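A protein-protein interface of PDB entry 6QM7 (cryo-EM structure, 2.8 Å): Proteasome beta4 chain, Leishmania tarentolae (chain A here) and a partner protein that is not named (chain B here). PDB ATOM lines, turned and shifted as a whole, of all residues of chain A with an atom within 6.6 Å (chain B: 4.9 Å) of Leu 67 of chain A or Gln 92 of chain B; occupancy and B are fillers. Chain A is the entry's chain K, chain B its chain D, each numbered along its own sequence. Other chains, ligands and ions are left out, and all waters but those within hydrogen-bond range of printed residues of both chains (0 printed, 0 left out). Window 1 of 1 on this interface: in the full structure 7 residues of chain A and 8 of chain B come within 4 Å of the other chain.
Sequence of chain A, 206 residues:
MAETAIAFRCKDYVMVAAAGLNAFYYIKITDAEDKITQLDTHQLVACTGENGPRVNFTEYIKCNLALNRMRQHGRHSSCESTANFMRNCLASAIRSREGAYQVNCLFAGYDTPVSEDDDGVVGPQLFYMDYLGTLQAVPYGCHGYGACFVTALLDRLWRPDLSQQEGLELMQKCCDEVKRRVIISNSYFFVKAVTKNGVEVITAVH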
ATOM      1  N   LYS A  62      -7.879 -21.753 -10.429  1.00  0.00           N
ATOM      2  CA  LYS A  62      -6.565 -21.257 -10.908  1.00  0.00           C
ATOM      3  C   LYS A  62      -6.722 -20.685 -12.317  1.00  0.00           C
ATOM      4  O   LYS A  62      -6.157 -19.612 -12.591  1.00  0.00           O
ATOM      5  CB  LYS A  62      -5.569 -22.412 -10.900  1.00  0.00           C
ATOM      6  CG  LYS A  62      -4.105 -22.066 -11.119  1.00  0.00           C
ATOM      7  CD  LYS A  62      -3.319 -23.275 -11.631  1.00  0.00           C
ATOM      8  CE  LYS A  62      -1.956 -23.444 -10.987  1.00  0.00           C
ATOM      9  NZ  LYS A  62      -1.128 -22.217 -11.116  1.00  0.00           N
ATOM     10  N   CYS A  63      -7.471 -21.384 -13.168  1.00  0.00           N
ATOM     11  CA  CYS A  63      -7.686 -21.031 -14.591  1.00  0.00           C
ATOM     12  C   CYS A  63      -8.608 -19.820 -14.683  1.00  0.00           C
ATOM     13  O   CYS A  63      -8.285 -18.902 -15.437  1.00  0.00           O
ATOM     14  CB  CYS A  63      -8.241 -22.215 -15.369  1.00  0.00           C
ATOM     15  SG  CYS A  63      -7.082 -23.615 -15.406  1.00  0.00           S
ATOM     16  N   ASN A  64      -9.688 -19.781 -13.908  1.00  0.00           N
ATOM     17  CA  ASN A  64     -10.580 -18.596 -13.868  1.00  0.00           C
ATOM     18  C   ASN A  64      -9.818 -17.395 -13.310  1.00  0.00           C
ATOM     19  O   ASN A  64      -9.998 -16.303 -13.866  1.00  0.00           O
ATOM     20  CB  ASN A  64     -11.872 -18.870 -13.118  1.00  0.00           C
ATOM     21  CG  ASN A  64     -12.845 -19.619 -13.991  1.00  0.00           C
ATOM     22  OD1 ASN A  64     -13.734 -19.012 -14.579  1.00  0.00           O
ATOM     23  ND2 ASN A  64     -12.648 -20.918 -14.135  1.00  0.00           N
ATOM     24  N   LEU A  65      -8.979 -17.568 -12.292  1.00  0.00           N
ATOM     25  CA  LEU A  65      -8.159 -16.447 -11.768  1.00  0.00           C
ATOM     26  C   LEU A  65      -7.221 -15.940 -12.856  1.00  0.00           C
ATOM     27  O   LEU A  65      -7.035 -14.715 -12.923  1.00  0.00           O
ATOM     28  CB  LEU A  65      -7.327 -16.879 -10.552  1.00  0.00           C
ATOM     29  CG  LEU A  65      -8.071 -17.042  -9.232  1.00  0.00           C
ATOM     30  CD1 LEU A  65      -7.079 -17.057  -8.085  1.00  0.00           C
ATOM     31  CD2 LEU A  65      -9.121 -15.950  -9.027  1.00  0.00           C
ATOM     32  N   ALA A  66      -6.584 -16.848 -13.593  1.00  0.00           N
ATOM     33  CA  ALA A  66      -5.602 -16.512 -14.647  1.00  0.00           C
ATOM     34  C   ALA A  66      -6.339 -15.820 -15.785  1.00  0.00           C
ATOM     35  O   ALA A  66      -5.819 -14.809 -16.285  1.00  0.00           O
ATOM     36  CB  ALA A  66      -4.891 -17.747 -15.131  1.00  0.00           C
ATOM     37  N   LEU A  67      -7.512 -16.345 -16.156  1.00  0.00           N
ATOM     38  CA  LEU A  67      -8.387 -15.751 -17.198  1.00  0.00           C
ATOM     39  C   LEU A  67      -8.755 -14.331 -16.779  1.00  0.00           C
ATOM     40  O   LEU A  67      -8.654 -13.433 -17.626  1.00  0.00           O
ATOM     41  CB  LEU A  67      -9.654 -16.594 -17.349  1.00  0.00           C
ATOM     42  CG  LEU A  67     -10.632 -16.118 -18.420  1.00  0.00           C
ATOM     43  CD1 LEU A  67      -9.914 -15.898 -19.737  1.00  0.00           C
ATOM     44  CD2 LEU A  67     -11.766 -17.112 -18.589  1.00  0.00           C
ATOM     45  N   ASN A  68      -9.179 -14.155 -15.524  1.00  0.00           N
ATOM     46  CA  ASN A  68      -9.573 -12.838 -14.968  1.00  0.00           C
ATOM     47  C   ASN A  68      -8.369 -11.896 -14.975  1.00  0.00           C
ATOM     48  O   ASN A  68      -8.610 -10.719 -15.120  1.00  0.00           O
ATOM     49  CB  ASN A  68     -10.220 -12.963 -13.590  1.00  0.00           C
ATOM     50  CG  ASN A  68     -11.583 -13.625 -13.647  1.00  0.00           C
ATOM     51  OD1 ASN A  68     -12.121 -13.834 -14.730  1.00  0.00           O
ATOM     52  ND2 ASN A  68     -12.131 -13.990 -12.495  1.00  0.00           N
ATOM     53  N   ARG A  69      -7.133 -12.373 -14.867  1.00  0.00           N
ATOM     54  CA  ARG A  69      -5.941 -11.495 -14.997  1.00  0.00           C
ATOM     55  C   ARG A  69      -5.740 -11.088 -16.464  1.00  0.00           C
ATOM     56  O   ARG A  69      -5.372  -9.921 -16.713  1.00  0.00           O
ATOM     57  CB  ARG A  69      -4.659 -12.174 -14.518  1.00  0.00           C
ATOM     58  CG  ARG A  69      -4.491 -12.217 -13.014  1.00  0.00           C
ATOM     59  CD  ARG A  69      -3.068 -12.631 -12.679  1.00  0.00           C
ATOM     60  NE  ARG A  69      -2.746 -14.026 -12.993  1.00  0.00           N
ATOM     61  CZ  ARG A  69      -3.167 -15.101 -12.308  1.00  0.00           C
ATOM     62  NH1 ARG A  69      -2.780 -16.309 -12.694  1.00  0.00           N
ATOM     63  NH2 ARG A  69      -3.980 -14.982 -11.264  1.00  0.00           N
ATOM     64  N   MET A  70      -5.905 -12.035 -17.385  1.00  0.00           N
ATOM     65  CA  MET A  70      -5.711 -11.823 -18.846  1.00  0.00           C
ATOM     66  C   MET A  70      -6.665 -10.723 -19.332  1.00  0.00           C
ATOM     67  O   MET A  70      -6.223  -9.852 -20.119  1.00  0.00           O
ATOM     68  CB  MET A  70      -5.965 -13.124 -19.629  1.00  0.00           C
ATOM     69  CG  MET A  70      -4.726 -13.744 -20.256  1.00  0.00           C
ATOM     70  SD  MET A  70      -3.211 -13.603 -19.259  1.00  0.00           S
ATOM     71  CE  MET A  70      -3.212 -15.163 -18.372  1.00  0.00           C
ATOM     72  N   ARG A  71      -7.918 -10.775 -18.872  1.00  0.00           N
ATOM     73  CA  ARG A  71      -9.005  -9.833 -19.240  1.00  0.00           C
ATOM     74  C   ARG A  71      -8.880  -8.527 -18.448  1.00  0.00           C
ATOM     75  O   ARG A  71      -9.366  -7.497 -18.943  1.00  0.00           O
ATOM     76  CB  ARG A  71     -10.357 -10.503 -18.998  1.00  0.00           C
ATOM     77  CG  ARG A  71     -10.658 -11.627 -19.979  1.00  0.00           C
ATOM     78  CD  ARG A  71     -11.927 -12.350 -19.595  1.00  0.00           C
ATOM     79  NE  ARG A  71     -12.409 -13.190 -20.679  1.00  0.00           N
ATOM     80  CZ  ARG A  71     -13.369 -14.108 -20.555  1.00  0.00           C
ATOM     81  NH1 ARG A  71     -13.964 -14.318 -19.387  1.00  0.00           N
ATOM     82  NH2 ARG A  71     -13.731 -14.826 -21.609  1.00  0.00           N
ATOM     83  N   GLN A  72      -8.252  -8.557 -17.277  1.00  0.00           N
ATOM     84  CA  GLN A  72      -8.029  -7.371 -16.413  1.00  0.00           C
ATOM     85  C   GLN A  72      -6.579  -6.891 -16.571  1.00  0.00           C
ATOM     86  O   GLN A  72      -6.021  -6.377 -15.582  1.00  0.00           O
ATOM     87  CB  GLN A  72      -8.404  -7.719 -14.963  1.00  0.00           C
ATOM     88  CG  GLN A  72      -9.897  -8.008 -14.777  1.00  0.00           C
ATOM     89  CD  GLN A  72     -10.277  -8.754 -13.518  1.00  0.00           C
ATOM     90  OE1 GLN A  72      -9.591  -8.691 -12.501  1.00  0.00           O
ATOM     91  NE2 GLN A  72     -11.395  -9.464 -13.578  1.00  0.00           N
ATOM     92  N   VAL B  65      -2.788 -12.957 -24.583  1.00  0.00           N
ATOM     93  CA  VAL B  65      -3.793 -14.050 -24.670  1.00  0.00           C
ATOM     94  C   VAL B  65      -3.529 -15.059 -23.547  1.00  0.00           C
ATOM     95  O   VAL B  65      -4.499 -15.560 -22.935  1.00  0.00           O
ATOM     96  CB  VAL B  65      -3.736 -14.715 -26.053  1.00  0.00           C
ATOM     97  CG1 VAL B  65      -4.699 -15.882 -26.131  1.00  0.00           C
ATOM     98  CG2 VAL B  65      -3.984 -13.721 -27.174  1.00  0.00           C
ATOM     99  N   ASP B  66      -2.264 -15.395 -23.328  1.00  0.00           N
ATOM    100  CA  ASP B  66      -1.801 -16.234 -22.193  1.00  0.00           C
ATOM    101  C   ASP B  66      -0.344 -15.861 -21.919  1.00  0.00           C
ATOM    102  O   ASP B  66       0.206 -15.098 -22.727  1.00  0.00           O
ATOM    103  CB  ASP B  66      -1.980 -17.725 -22.495  1.00  0.00           C
ATOM    104  CG  ASP B  66      -2.138 -18.616 -21.266  1.00  0.00           C
ATOM    105  OD1 ASP B  66      -1.981 -18.105 -20.129  1.00  0.00           O
ATOM    106  OD2 ASP B  66      -2.414 -19.829 -21.450  1.00  0.00           O
ATOM    107  N   GLN B  88      -8.356 -15.769 -25.090  1.00  0.00           N
ATOM    108  CA  GLN B  88      -7.977 -15.768 -23.656  1.00  0.00           C
ATOM    109  C   GLN B  88      -8.713 -16.896 -22.934  1.00  0.00           C
ATOM    110  O   GLN B  88      -8.073 -17.578 -22.097  1.00  0.00           O
ATOM    111  CB  GLN B  88      -8.277 -14.413 -23.019  1.00  0.00           C
ATOM    112  CG  GLN B  88      -7.219 -13.385 -23.365  1.00  0.00           C
ATOM    113  CD  GLN B  88      -7.604 -11.979 -23.009  1.00  0.00           C
ATOM    114  OE1 GLN B  88      -8.735 -11.696 -22.641  1.00  0.00           O
ATOM    115  NE2 GLN B  88      -6.646 -11.084 -23.115  1.00  0.00           N
ATOM    116  N   LEU B  89      -9.996 -17.066 -23.240  1.00  0.00           N
ATOM    117  CA  LEU B  89     -10.840 -18.113 -22.627  1.00  0.00           C
ATOM    118  C   LEU B  89     -10.386 -19.480 -23.131  1.00  0.00           C
ATOM    119  O   LEU B  89     -10.392 -20.413 -22.328  1.00  0.00           O
ATOM    120  CB  LEU B  89     -12.310 -17.846 -22.966  1.00  0.00           C
ATOM    121  CG  LEU B  89     -13.310 -18.924 -22.537  1.00  0.00           C
ATOM    122  CD1 LEU B  89     -13.213 -19.228 -21.041  1.00  0.00           C
ATOM    123  CD2 LEU B  89     -14.734 -18.507 -22.894  1.00  0.00           C
ATOM    124  N   GLU B  90     -10.046 -19.594 -24.417  1.00  0.00           N
ATOM    125  CA  GLU B  90      -9.702 -20.886 -25.066  1.00  0.00           C
ATOM    126  C   GLU B  90      -8.392 -21.407 -24.487  1.00  0.00           C
ATOM    127  O   GLU B  90      -8.312 -22.614 -24.240  1.00  0.00           O
ATOM    128  CB  GLU B  90      -9.596 -20.752 -26.584  1.00  0.00           C
ATOM    129  CG  GLU B  90      -9.003 -21.976 -27.273  1.00  0.00           C
ATOM    130  CD  GLU B  90      -9.749 -23.298 -27.093  1.00  0.00           C
ATOM    131  OE1 GLU B  90      -9.144 -24.347 -27.421  1.00  0.00           O
ATOM    132  OE2 GLU B  90     -10.930 -23.288 -26.638  1.00  0.00           O
ATOM    133  N   CYS B  91      -7.402 -20.542 -24.310  1.00  0.00           N
ATOM    134  CA  CYS B  91      -6.113 -20.906 -23.671  1.00  0.00           C
ATOM    135  C   CYS B  91      -6.340 -21.442 -22.256  1.00  0.00           C
ATOM    136  O   CYS B  91      -5.626 -22.369 -21.850  1.00  0.00           O
ATOM    137  CB  CYS B  91      -5.177 -19.718 -23.608  1.00  0.00           C
ATOM    138  SG  CYS B  91      -4.458 -19.342 -25.222  1.00  0.00           S
ATOM    139  N   GLN B  92      -7.291 -20.876 -21.531  1.00  0.00           N
ATOM    140  CA  GLN B  92      -7.594 -21.293 -20.146  1.00  0.00           C
ATOM    141  C   GLN B  92      -8.473 -22.552 -20.192  1.00  0.00           C
ATOM    142  O   GLN B  92      -8.248 -23.428 -19.347  1.00  0.00           O
ATOM    143  CB  GLN B  92      -8.152 -20.096 -19.374  1.00  0.00           C
ATOM    144  CG  GLN B  92      -7.211 -19.585 -18.287  1.00  0.00           C
ATOM    145  CD  GLN B  92      -5.831 -19.147 -18.712  1.00  0.00           C
ATOM    146  OE1 GLN B  92      -4.833 -19.545 -18.115  1.00  0.00           O
ATOM    147  NE2 GLN B  92      -5.769 -18.286 -19.722  1.00  0.00           N
ATOM    148  N   ARG B  93      -9.409 -22.661 -21.139  1.00  0.00           N
ATOM    149  CA  ARG B  93     -10.226 -23.890 -21.349  1.00  0.00           C
ATOM    150  C   ARG B  93      -9.299 -25.053 -21.699  1.00  0.00           C
ATOM    151  O   ARG B  93      -9.620 -26.188 -21.349  1.00  0.00           O
ATOM    152  CB  ARG B  93     -11.270 -23.719 -22.459  1.00  0.00           C
ATOM    153  CG  ARG B  93     -12.336 -24.814 -22.520  1.00  0.00           C
ATOM    154  CD  ARG B  93     -12.883 -25.101 -23.915  1.00  0.00           C
ATOM    155  NE  ARG B  93     -11.784 -25.354 -24.846  1.00  0.00           N
ATOM    156  CZ  ARG B  93     -11.112 -26.503 -24.965  1.00  0.00           C
ATOM    157  NH1 ARG B  93     -11.434 -27.562 -24.233  1.00  0.00           N
ATOM    158  NH2 ARG B  93     -10.112 -26.588 -25.832  1.00  0.00           N
ATOM    159  N   PHE B  94      -8.188 -24.768 -22.364  1.00  0.00           N
ATOM    160  CA  PHE B  94      -7.201 -25.770 -22.826  1.00  0.00           C
ATOM    161  C   PHE B  94      -6.317 -26.233 -21.657  1.00  0.00           C
ATOM    162  O   PHE B  94      -6.044 -27.424 -21.569  1.00  0.00           O
ATOM    163  CB  PHE B  94      -6.382 -25.157 -23.957  1.00  0.00           C
ATOM    164  CG  PHE B  94      -5.363 -26.088 -24.531  1.00  0.00           C
ATOM    165  CD1 PHE B  94      -5.619 -26.769 -25.706  1.00  0.00           C
ATOM    166  CD2 PHE B  94      -4.165 -26.301 -23.883  1.00  0.00           C
ATOM    167  CE1 PHE B  94      -4.678 -27.639 -26.236  1.00  0.00           C
ATOM    168  CE2 PHE B  94      -3.227 -27.174 -24.408  1.00  0.00           C
ATOM    169  CZ  PHE B  94      -3.483 -27.841 -25.587  1.00  0.00           C
ATOM    170  N   SER B  95      -5.828 -25.315 -20.823  1.00  0.00           N
ATOM    171  CA  SER B  95      -5.071 -25.643 -19.584  1.00  0.00           C
ATOM    172  C   SER B  95      -5.940 -26.488 -18.636  1.00  0.00           C
ATOM    173  O   SER B  95      -5.402 -27.413 -18.006  1.00  0.00           O
ATOM    174  CB  SER B  95      -4.545 -24.405 -18.908  1.00  0.00           C
ATOM    175  OG  SER B  95      -3.456 -23.876 -19.651  1.00  0.00           O
ATOM    176  N   LEU B  96      -7.237 -26.197 -18.559  1.00  0.00           N
ATOM    177  CA  LEU B  96      -8.210 -26.985 -17.759  1.00  0.00           C
ATOM    178  C   LEU B  96      -8.310 -28.413 -18.282  1.00  0.00           C
ATOM    179  O   LEU B  96      -8.367 -29.333 -17.440  1.00  0.00           O
ATOM    180  CB  LEU B  96      -9.598 -26.350 -17.817  1.00  0.00           C
ATOM    181  CG  LEU B  96     -10.071 -25.701 -16.529  1.00  0.00           C
ATOM    182  CD1 LEU B  96     -11.505 -25.219 -16.699  1.00  0.00           C
ATOM    183  CD2 LEU B  96      -9.944 -26.658 -15.349  1.00  0.00           C
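Lys 62 of chain A touches none of the printed residues of chain B. Of chain B, only Gln 88, Leu 89 and Gln 92 come within 4 Å of Leu 67 of chain A. Printed residues of chain B within 4 Å of Arg 71 of chain A: Gln 88 and Leu 89. Printed residues of chain A within 4 Å of Gln 88 of chain B: Leu 67, Met 70 and Arg 71. Gln 92 of chain B touches just these residues of chain A: Cys 63 (3.1 Å), Ala 66 (3.5 Å) and Leu 67 (3.9 Å). Arg 93 of chain B touches none of the printed residues of chain A. Of the printed residues of chain A, Leu 96 of chain B touches Cys 63 (3.8 Å). The nearest printed residue of chain B that does not touch Leu 67 of chain A is Glu 90 of chain B (6.0 Å). The nearest residue of chain A that does not touch Gln 92 of chain B is Met 70 of chain A (4.3 Å). The nearest printed residue of chain B that does not touch Ala 66 of chain A is Asp 66 of chain B (5.8 Å).
Among the printed residues, merely in contact across the chains: Cys 63 of chain A with Gln 92 of chain B, Cys 63 of chain A with Leu 96 of chain B, Ala 66 of chain A with Gln 92 of chain B, Leu 67 of chain A with Gln 88 of chain B, Leu 67 of chain A with Leu 89 of chain B, Leu 67 of chain A with Gln 92 of chain B, Met 70 of chain A with Val 65 of chain B, Met 70 of chain A with Asp 66 of chain B, Arg 71 of chain A with Gln 88 of chain B and Arg 71 of chain A with Leu 89 of chain B.
Hydrophobic or aromatic side chains of chain A within 4 Å of the printed part of chain B: Ala 66, Leu 67 and Met 70. Along chain A the printed residues that touch a printed residue of chain B span positions 63 to 71. Of the 11 printed residues of chain B, 6 touch a printed residue of chain A. Hydrophobic or aromatic side chains of chain B that line the printed part of chain A: Leu 89 and Leu 96. Among the printed residues, 11 pairs touch across the chains.
The backbone carbonyl oxygen of Met 70 of chain A is in hydrogen-bond range of the side-chain amide nitrogen of Gln 88 of chain B (3.3 Å).
O of Gln 88 of chain B sits at hydrogen-bond distance from NE2 of Gln 92 of chain B, at 3.4 Å.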
